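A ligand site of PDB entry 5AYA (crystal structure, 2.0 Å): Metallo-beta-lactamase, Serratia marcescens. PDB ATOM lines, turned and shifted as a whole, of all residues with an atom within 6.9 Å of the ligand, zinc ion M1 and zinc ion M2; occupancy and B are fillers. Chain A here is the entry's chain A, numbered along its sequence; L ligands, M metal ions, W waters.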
ATOM      1  N   TRP A   5      -3.535 -13.223  21.288  1.00  0.00           N
ATOM      2  CA  TRP A   5      -4.899 -13.685  21.145  1.00  0.00           C
ATOM      3  C   TRP A   5      -5.604 -13.051  19.928  1.00  0.00           C
ATOM      4  O   TRP A   5      -6.605 -13.590  19.444  1.00  0.00           O
ATOM      5  CB  TRP A   5      -5.706 -13.376  22.423  1.00  0.00           C
ATOM      6  CG  TRP A   5      -5.187 -14.062  23.682  1.00  0.00           C
ATOM      7  CD1 TRP A   5      -4.311 -15.126  23.756  1.00  0.00           C
ATOM      8  CD2 TRP A   5      -5.571 -13.770  25.037  1.00  0.00           C
ATOM      9  NE1 TRP A   5      -4.123 -15.496  25.071  1.00  0.00           N
ATOM     10  CE2 TRP A   5      -4.886 -14.689  25.880  1.00  0.00           C
ATOM     11  CE3 TRP A   5      -6.423 -12.824  25.624  1.00  0.00           C
ATOM     12  CZ2 TRP A   5      -5.028 -14.685  27.266  1.00  0.00           C
ATOM     13  CZ3 TRP A   5      -6.556 -12.816  27.021  1.00  0.00           C
ATOM     14  CH2 TRP A   5      -5.840 -13.733  27.824  1.00  0.00           C
ATOM     15  N   ILE A  26      -5.669 -18.212  19.927  1.00  0.00           N
ATOM     16  CA  ILE A  26      -6.978 -18.752  20.331  1.00  0.00           C
ATOM     17  C   ILE A  26      -7.630 -19.510  19.181  1.00  0.00           C
ATOM     18  O   ILE A  26      -7.687 -19.001  18.076  1.00  0.00           O
ATOM     19  CB  ILE A  26      -7.939 -17.621  20.753  1.00  0.00           C
ATOM     20  CG1 ILE A  26      -7.364 -16.823  21.925  1.00  0.00           C
ATOM     21  CG2 ILE A  26      -9.315 -18.180  21.125  1.00  0.00           C
ATOM     22  CD1 ILE A  26      -7.463 -17.531  23.257  1.00  0.00           C
ATOM     23  N   HIS A  72     -17.020 -20.659  26.028  1.00  0.00           N
ATOM     24  CA  HIS A  72     -17.379 -19.832  27.195  1.00  0.00           C
ATOM     25  C   HIS A  72     -17.100 -18.331  27.040  1.00  0.00           C
ATOM     26  O   HIS A  72     -16.326 -17.909  26.159  1.00  0.00           O
ATOM     27  CB  HIS A  72     -16.669 -20.363  28.433  1.00  0.00           C
ATOM     28  CG  HIS A  72     -15.217 -20.064  28.467  1.00  0.00           C
ATOM     29  ND1 HIS A  72     -14.258 -20.940  27.984  1.00  0.00           N
ATOM     30  CD2 HIS A  72     -14.544 -18.977  28.903  1.00  0.00           C
ATOM     31  CE1 HIS A  72     -13.069 -20.378  28.078  1.00  0.00           C
ATOM     32  NE2 HIS A  72     -13.216 -19.198  28.659  1.00  0.00           N
ATOM     33  N   SER A  73     -17.622 -17.555  27.987  1.00  0.00           N
ATOM     34  CA  SER A  73     -17.867 -16.116  27.780  1.00  0.00           C
ATOM     35  C   SER A  73     -16.808 -15.272  28.457  1.00  0.00           C
ATOM     36  O   SER A  73     -17.118 -14.375  29.238  1.00  0.00           O
ATOM     37  CB  SER A  73     -19.254 -15.738  28.328  1.00  0.00           C
ATOM     38  OG  SER A  73     -19.457 -16.270  29.625  1.00  0.00           O
ATOM     39  N   HIS A  74     -15.544 -15.621  28.237  1.00  0.00           N
ATOM     40  CA  HIS A  74     -14.453 -14.710  28.495  1.00  0.00           C
ATOM     41  C   HIS A  74     -14.039 -14.031  27.213  1.00  0.00           C
ATOM     42  O   HIS A  74     -14.205 -14.611  26.127  1.00  0.00           O
ATOM     43  CB  HIS A  74     -13.265 -15.444  29.064  1.00  0.00           C
ATOM     44  CG  HIS A  74     -13.497 -15.941  30.442  1.00  0.00           C
ATOM     45  ND1 HIS A  74     -12.630 -16.789  31.079  1.00  0.00           N
ATOM     46  CD2 HIS A  74     -14.481 -15.668  31.325  1.00  0.00           C
ATOM     47  CE1 HIS A  74     -13.097 -17.067  32.282  1.00  0.00           C
ATOM     48  NE2 HIS A  74     -14.214 -16.393  32.466  1.00  0.00           N
ATOM     49  N   GLU A  75     -13.510 -12.825  27.355  1.00  0.00           N
ATOM     50  CA  GLU A  75     -13.240 -11.905  26.246  1.00  0.00           C
ATOM     51  C   GLU A  75     -12.425 -12.531  25.101  1.00  0.00           C
ATOM     52  O   GLU A  75     -12.736 -12.335  23.913  1.00  0.00           O
ATOM     53  CB  GLU A  75     -12.547 -10.644  26.787  1.00  0.00           C
ATOM     54  CG  GLU A  75     -11.199 -10.909  27.464  1.00  0.00           C
ATOM     55  CD  GLU A  75     -10.580  -9.664  28.109  1.00  0.00           C
ATOM     56  OE1 GLU A  75     -11.018  -8.530  27.791  1.00  0.00           O
ATOM     57  OE2 GLU A  75      -9.617  -9.822  28.905  1.00  0.00           O
ATOM     58  N   ASP A  76     -11.431 -13.324  25.469  1.00  0.00           N
ATOM     59  CA  ASP A  76     -10.500 -13.911  24.523  1.00  0.00           C
ATOM     60  C   ASP A  76     -11.109 -14.980  23.571  1.00  0.00           C
ATOM     61  O   ASP A  76     -10.500 -15.258  22.528  1.00  0.00           O
ATOM     62  CB  ASP A  76      -9.244 -14.464  25.231  1.00  0.00           C
ATOM     63  CG  ASP A  76      -9.548 -15.541  26.260  1.00  0.00           C
ATOM     64  OD1 ASP A  76     -10.645 -15.516  26.884  1.00  0.00           O
ATOM     65  OD2 ASP A  76      -8.638 -16.346  26.529  1.00  0.00           O
ATOM     66  N   HIS A  77     -12.282 -15.526  23.906  1.00  0.00           N
ATOM     67  CA  HIS A  77     -13.004 -16.454  23.004  1.00  0.00           C
ATOM     68  C   HIS A  77     -14.256 -15.834  22.433  1.00  0.00           C
ATOM     69  O   HIS A  77     -14.702 -16.224  21.355  1.00  0.00           O
ATOM     70  CB  HIS A  77     -13.418 -17.722  23.756  1.00  0.00           C
ATOM     71  CG  HIS A  77     -12.309 -18.334  24.531  1.00  0.00           C
ATOM     72  ND1 HIS A  77     -11.271 -19.017  23.931  1.00  0.00           N
ATOM     73  CD2 HIS A  77     -11.993 -18.252  25.852  1.00  0.00           C
ATOM     74  CE1 HIS A  77     -10.403 -19.399  24.853  1.00  0.00           C
ATOM     75  NE2 HIS A  77     -10.780 -18.875  26.009  1.00  0.00           N
ATOM     76  N   ASP A 111     -18.720 -15.423  37.993  1.00  0.00           N
ATOM     77  CA  ASP A 111     -17.581 -15.809  37.161  1.00  0.00           C
ATOM     78  C   ASP A 111     -16.265 -15.674  37.940  1.00  0.00           C
ATOM     79  O   ASP A 111     -16.008 -14.660  38.602  1.00  0.00           O
ATOM     80  CB  ASP A 111     -17.538 -14.947  35.901  1.00  0.00           C
ATOM     81  CG  ASP A 111     -16.759 -15.606  34.763  1.00  0.00           C
ATOM     82  OD1 ASP A 111     -17.366 -16.404  34.020  1.00  0.00           O
ATOM     83  OD2 ASP A 111     -15.544 -15.358  34.633  1.00  0.00           O
ATOM     84  N   GLN A 113     -13.483 -14.942  36.880  1.00  0.00           N
ATOM     85  CA  GLN A 113     -12.715 -13.817  36.333  1.00  0.00           C
ATOM     86  C   GLN A 113     -13.551 -12.558  36.127  1.00  0.00           C
ATOM     87  O   GLN A 113     -13.137 -11.652  35.405  1.00  0.00           O
ATOM     88  CB  GLN A 113     -12.053 -14.230  35.022  1.00  0.00           C
ATOM     89  CG  GLN A 113     -11.070 -15.375  35.195  1.00  0.00           C
ATOM     90  CD  GLN A 113     -10.295 -15.673  33.932  1.00  0.00           C
ATOM     91  OE1 GLN A 113     -10.112 -14.805  33.084  1.00  0.00           O
ATOM     92  NE2 GLN A 113      -9.897 -16.918  33.765  1.00  0.00           N
ATOM     93  N   LEU A 117     -10.997 -10.037  34.150  1.00  0.00           N
ATOM     94  CA  LEU A 117     -11.300  -9.820  32.735  1.00  0.00           C
ATOM     95  C   LEU A 117     -12.256  -8.652  32.557  1.00  0.00           C
ATOM     96  O   LEU A 117     -13.443  -8.744  32.893  1.00  0.00           O
ATOM     97  CB  LEU A 117     -11.919 -11.071  32.104  1.00  0.00           C
ATOM     98  CG  LEU A 117     -11.027 -12.310  31.961  1.00  0.00           C
ATOM     99  CD1 LEU A 117     -11.420 -13.085  30.726  1.00  0.00           C
ATOM    100  CD2 LEU A 117      -9.537 -11.960  31.909  1.00  0.00           C
ATOM    101  N   HIS A 150     -15.061 -23.519  34.847  1.00  0.00           N
ATOM    102  CA  HIS A 150     -14.245 -22.369  34.487  1.00  0.00           C
ATOM    103  C   HIS A 150     -15.202 -21.195  34.296  1.00  0.00           C
ATOM    104  O   HIS A 150     -14.854 -20.048  34.587  1.00  0.00           O
ATOM    105  CB  HIS A 150     -13.435 -22.694  33.193  1.00  0.00           C
ATOM    106  CG  HIS A 150     -12.587 -21.573  32.666  1.00  0.00           C
ATOM    107  ND1 HIS A 150     -11.254 -21.458  32.989  1.00  0.00           N
ATOM    108  CD2 HIS A 150     -12.821 -20.647  31.706  1.00  0.00           C
ATOM    109  CE1 HIS A 150     -10.728 -20.444  32.328  1.00  0.00           C
ATOM    110  NE2 HIS A 150     -11.651 -19.929  31.539  1.00  0.00           N
ATOM    111  N   THR A 151     -16.361 -21.504  33.703  1.00  0.00           N
ATOM    112  CA  THR A 151     -17.527 -20.626  33.691  1.00  0.00           C
ATOM    113  C   THR A 151     -18.738 -21.521  33.943  1.00  0.00           C
ATOM    114  O   THR A 151     -18.654 -22.745  33.739  1.00  0.00           O
ATOM    115  CB  THR A 151     -17.763 -19.911  32.346  1.00  0.00           C
ATOM    116  OG1 THR A 151     -18.078 -20.886  31.340  1.00  0.00           O
ATOM    117  CG2 THR A 151     -16.535 -19.072  31.913  1.00  0.00           C
ATOM    118  N   ASP A 174     -13.707 -27.023  25.628  1.00  0.00           N
ATOM    119  CA  ASP A 174     -13.738 -25.815  26.442  1.00  0.00           C
ATOM    120  C   ASP A 174     -12.619 -25.878  27.466  1.00  0.00           C
ATOM    121  O   ASP A 174     -12.096 -26.949  27.750  1.00  0.00           O
ATOM    122  CB  ASP A 174     -15.077 -25.694  27.160  1.00  0.00           C
ATOM    123  CG  ASP A 174     -15.376 -24.260  27.635  1.00  0.00           C
ATOM    124  OD1 ASP A 174     -14.658 -23.325  27.207  1.00  0.00           O
ATOM    125  OD2 ASP A 174     -16.252 -24.099  28.489  1.00  0.00           O
ATOM    126  N   SER A 175     -12.247 -24.707  28.014  1.00  0.00           N
ATOM    127  CA  SER A 175     -11.236 -24.655  29.075  1.00  0.00           C
ATOM    128  C   SER A 175     -11.776 -25.294  30.332  1.00  0.00           C
ATOM    129  O   SER A 175     -12.917 -25.034  30.751  1.00  0.00           O
ATOM    130  CB  SER A 175     -10.790 -23.207  29.375  1.00  0.00           C
ATOM    131  OG  SER A 175     -10.600 -22.477  28.171  1.00  0.00           O
ATOM    132  N   LEU A 176     -10.927 -26.090  30.972  1.00  0.00           N
ATOM    133  CA  LEU A 176     -11.237 -26.777  32.225  1.00  0.00           C
ATOM    134  C   LEU A 176     -10.312 -26.296  33.362  1.00  0.00           C
ATOM    135  O   LEU A 176     -10.176 -26.979  34.393  1.00  0.00           O
ATOM    136  CB  LEU A 176     -11.074 -28.276  32.021  1.00  0.00           C
ATOM    137  CG  LEU A 176     -11.918 -28.898  30.873  1.00  0.00           C
ATOM    138  CD1 LEU A 176     -11.538 -30.364  30.690  1.00  0.00           C
ATOM    139  CD2 LEU A 176     -13.401 -28.744  31.166  1.00  0.00           C
ATOM    140  N   THR A 177      -9.821 -25.079  33.234  1.00  0.00           N
ATOM    141  CA  THR A 177      -8.813 -24.528  34.136  1.00  0.00           C
ATOM    142  C   THR A 177      -9.438 -23.755  35.305  1.00  0.00           C
ATOM    143  O   THR A 177     -10.301 -22.877  35.112  1.00  0.00           O
ATOM    144  CB  THR A 177      -7.797 -23.644  33.373  1.00  0.00           C
ATOM    145  OG1 THR A 177      -8.456 -22.740  32.475  1.00  0.00           O
ATOM    146  CG2 THR A 177      -6.842 -24.526  32.586  1.00  0.00           C
ATOM    147  N   VAL A 179      -8.970 -21.027  37.160  1.00  0.00           N
ATOM    148  CA  VAL A 179      -8.297 -19.747  37.250  1.00  0.00           C
ATOM    149  C   VAL A 179      -9.347 -18.680  37.411  1.00  0.00           C
ATOM    150  O   VAL A 179     -10.493 -18.880  37.048  1.00  0.00           O
ATOM    151  CB  VAL A 179      -7.447 -19.446  36.004  1.00  0.00           C
ATOM    152  CG1 VAL A 179      -6.175 -20.281  36.012  1.00  0.00           C
ATOM    153  CG2 VAL A 179      -8.237 -19.690  34.731  1.00  0.00           C
ATOM    154  N   ALA A 214      -9.602 -24.866  23.210  1.00  0.00           N
ATOM    155  CA  ALA A 214      -9.906 -23.442  23.013  1.00  0.00           C
ATOM    156  C   ALA A 214      -8.601 -22.646  22.970  1.00  0.00           C
ATOM    157  O   ALA A 214      -8.377 -21.836  22.060  1.00  0.00           O
ATOM    158  CB  ALA A 214     -10.813 -22.942  24.136  1.00  0.00           C
ATOM    159  N   HIS A 215      -7.732 -22.917  23.940  1.00  0.00           N
ATOM    160  CA  HIS A 215      -6.307 -22.579  23.812  1.00  0.00           C
ATOM    161  C   HIS A 215      -5.534 -23.704  23.095  1.00  0.00           C
ATOM    162  O   HIS A 215      -5.270 -24.768  23.659  1.00  0.00           O
ATOM    163  CB  HIS A 215      -5.704 -22.270  25.195  1.00  0.00           C
ATOM    164  CG  HIS A 215      -6.211 -20.988  25.803  1.00  0.00           C
ATOM    165  ND1 HIS A 215      -5.761 -19.743  25.419  1.00  0.00           N
ATOM    166  CD2 HIS A 215      -7.207 -20.777  26.694  1.00  0.00           C
ATOM    167  CE1 HIS A 215      -6.452 -18.814  26.059  1.00  0.00           C
ATOM    168  NE2 HIS A 215      -7.338 -19.410  26.837  1.00  0.00           N
ATOM    169  N   GLU A 217      -2.609 -24.623  22.057  1.00  0.00           N
ATOM    170  CA  GLU A 217      -1.441 -25.341  22.555  1.00  0.00           C
ATOM    171  C   GLU A 217      -1.768 -26.403  23.609  1.00  0.00           C
ATOM    172  O   GLU A 217      -0.988 -27.334  23.800  1.00  0.00           O
ATOM    173  CB  GLU A 217      -0.395 -24.354  23.091  1.00  0.00           C
ATOM    174  CG  GLU A 217      -0.657 -23.792  24.478  1.00  0.00           C
ATOM    175  CD  GLU A 217      -1.720 -22.724  24.489  1.00  0.00           C
ATOM    176  OE1 GLU A 217      -2.062 -22.201  23.406  1.00  0.00           O
ATOM    177  OE2 GLU A 217      -2.224 -22.415  25.586  1.00  0.00           O
ATOM    178  N   VAL A 218      -2.967 -26.353  24.183  1.00  0.00           N
ATOM    179  CA  VAL A 218      -3.342 -27.297  25.227  1.00  0.00           C
ATOM    180  C   VAL A 218      -3.465 -28.717  24.665  1.00  0.00           C
ATOM    181  O   VAL A 218      -3.365 -29.694  25.427  1.00  0.00           O
ATOM    182  CB  VAL A 218      -4.687 -26.895  25.897  1.00  0.00           C
ATOM    183  CG1 VAL A 218      -5.153 -27.954  26.883  1.00  0.00           C
ATOM    184  CG2 VAL A 218      -4.552 -25.541  26.607  1.00  0.00           C
ATOM    185  N   ARG A 252      -4.560 -29.163  37.660  1.00  0.00           N
ATOM    186  CA  ARG A 252      -4.582 -27.733  37.857  1.00  0.00           C
ATOM    187  C   ARG A 252      -5.508 -27.322  39.007  1.00  0.00           C
ATOM    188  O   ARG A 252      -5.226 -26.362  39.720  1.00  0.00           O
ATOM    189  CB  ARG A 252      -5.009 -27.036  36.562  1.00  0.00           C
ATOM    190  CG  ARG A 252      -4.986 -25.523  36.642  1.00  0.00           C
ATOM    191  CD  ARG A 252      -3.576 -24.978  36.826  1.00  0.00           C
ATOM    192  NE  ARG A 252      -3.478 -23.629  36.281  1.00  0.00           N
ATOM    193  CZ  ARG A 252      -3.422 -23.339  34.983  1.00  0.00           C
ATOM    194  NH1 ARG A 252      -3.348 -24.317  34.078  1.00  0.00           N
ATOM    195  NH2 ARG A 252      -3.410 -22.070  34.581  1.00  0.00           N
HETATM  196  O1  LIG L   1      -6.976 -21.639  30.329  1.00  0.00           O
HETATM  197  C1  LIG L   1      -6.420 -20.597  29.999  1.00  0.00           C
HETATM  198  C2  LIG L   1      -7.203 -19.303  30.040  1.00  0.00           C
HETATM  199  C3  LIG L   1      -8.661 -19.654  29.853  1.00  0.00           C
HETATM  200  S1  LIG L   1      -9.654 -18.218  29.470  1.00  0.00           S
HETATM  201  C4  LIG L   1      -6.958 -18.499  31.325  1.00  0.00           C
HETATM  202  N1  LIG L   1      -5.165 -20.508  29.533  1.00  0.00           N
HETATM  203  C5  LIG L   1      -4.363 -21.708  29.254  1.00  0.00           C
HETATM  204  C6  LIG L   1      -4.115 -22.538  30.469  1.00  0.00           C
HETATM  205  O2  LIG L   1      -3.918 -21.919  31.629  1.00  0.00           O
HETATM  206  O3  LIG L   1      -4.018 -23.754  30.379  1.00  0.00           O
HETATM  207  C7  LIG L   1      -4.444 -19.272  29.211  1.00  0.00           C
HETATM  208  C8  LIG L   1      -3.091 -19.693  28.642  1.00  0.00           C
HETATM  209  C9  LIG L   1      -3.013 -21.206  28.751  1.00  0.00           C
HETATM  210 ZN    ZN M   1     -11.794 -18.485  30.118  1.00  0.00          ZN
HETATM  211 ZN    ZN M   2      -9.205 -18.196  27.146  1.00  0.00          ZN
HETATM  212  O   HOH W   1      -7.143 -24.179  28.991  1.00  0.00           O
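Zinc ion M2 is bound by OD2 of Asp 76 (2.0 Å). Zinc ion M2 is bound by NE2 of His 77 (2.1 Å). A ring nitrogen (NE2) of His 215 binds zinc ion M2. Zinc ion M2 is bound by a sulfur (S1) of the ligand, 2.4 Å away.
Ser 175 touches the ligand. Val 179 touches the ligand. OE2 of Glu 217 touches C9 of the ligand (3.5 Å). Hydrophobic or aromatic side chains that line the ligand: His 150, Val 179 and His 215. Within 4 Å of the ligand: His 72, His 74, Asp 76, His 77, His 150, Ser 175, Thr 177, Val 179, His 215, Glu 217 and Arg 252. The nearest printed residue that does not touch the ligand is Gln 113 (4.1 Å).
Within 4 Å of zinc ion M1: His 72, His 74 and His 150. The nearest printed residue that does not touch zinc ion M1 is His 77 (4.3 Å).
The backbone carbonyl oxygen of Thr 177 sits at hydrogen-bond distance from a ring nitrogen (ND1) of His 150 (2.7 Å). A ring nitrogen (NE2) of His 74 is in hydrogen-bond range of the side-chain carboxylate (OD2) of Asp 111 (2.7 Å). ND1 of His 72 lies within hydrogen-bond range of OD1 of Asp 174, 2.5 Å away.
An oxygen (O1) of the ligand sits at hydrogen-bond distance from the side-chain hydroxyl of Thr 177 (2.8 Å). NH2 of Arg 252 is in salt-bridge range of O2 of the ligand, 3.0 Å away.
Zinc ion M1 is bound by a ring nitrogen (NE2) of His 150 (2.0 Å), a ring nitrogen (ND1) of His 74 (2.1 Å), a ring nitrogen (NE2) of His 72 (2.2 Å) and a sulfur (S1) of the ligand (2.3 Å).
Within 4 Å of zinc ion M2: Asp 76, His 77 and His 215. The nearest printed residue that does not touch zinc ion M2 is Ile 26 (4.3 Å).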
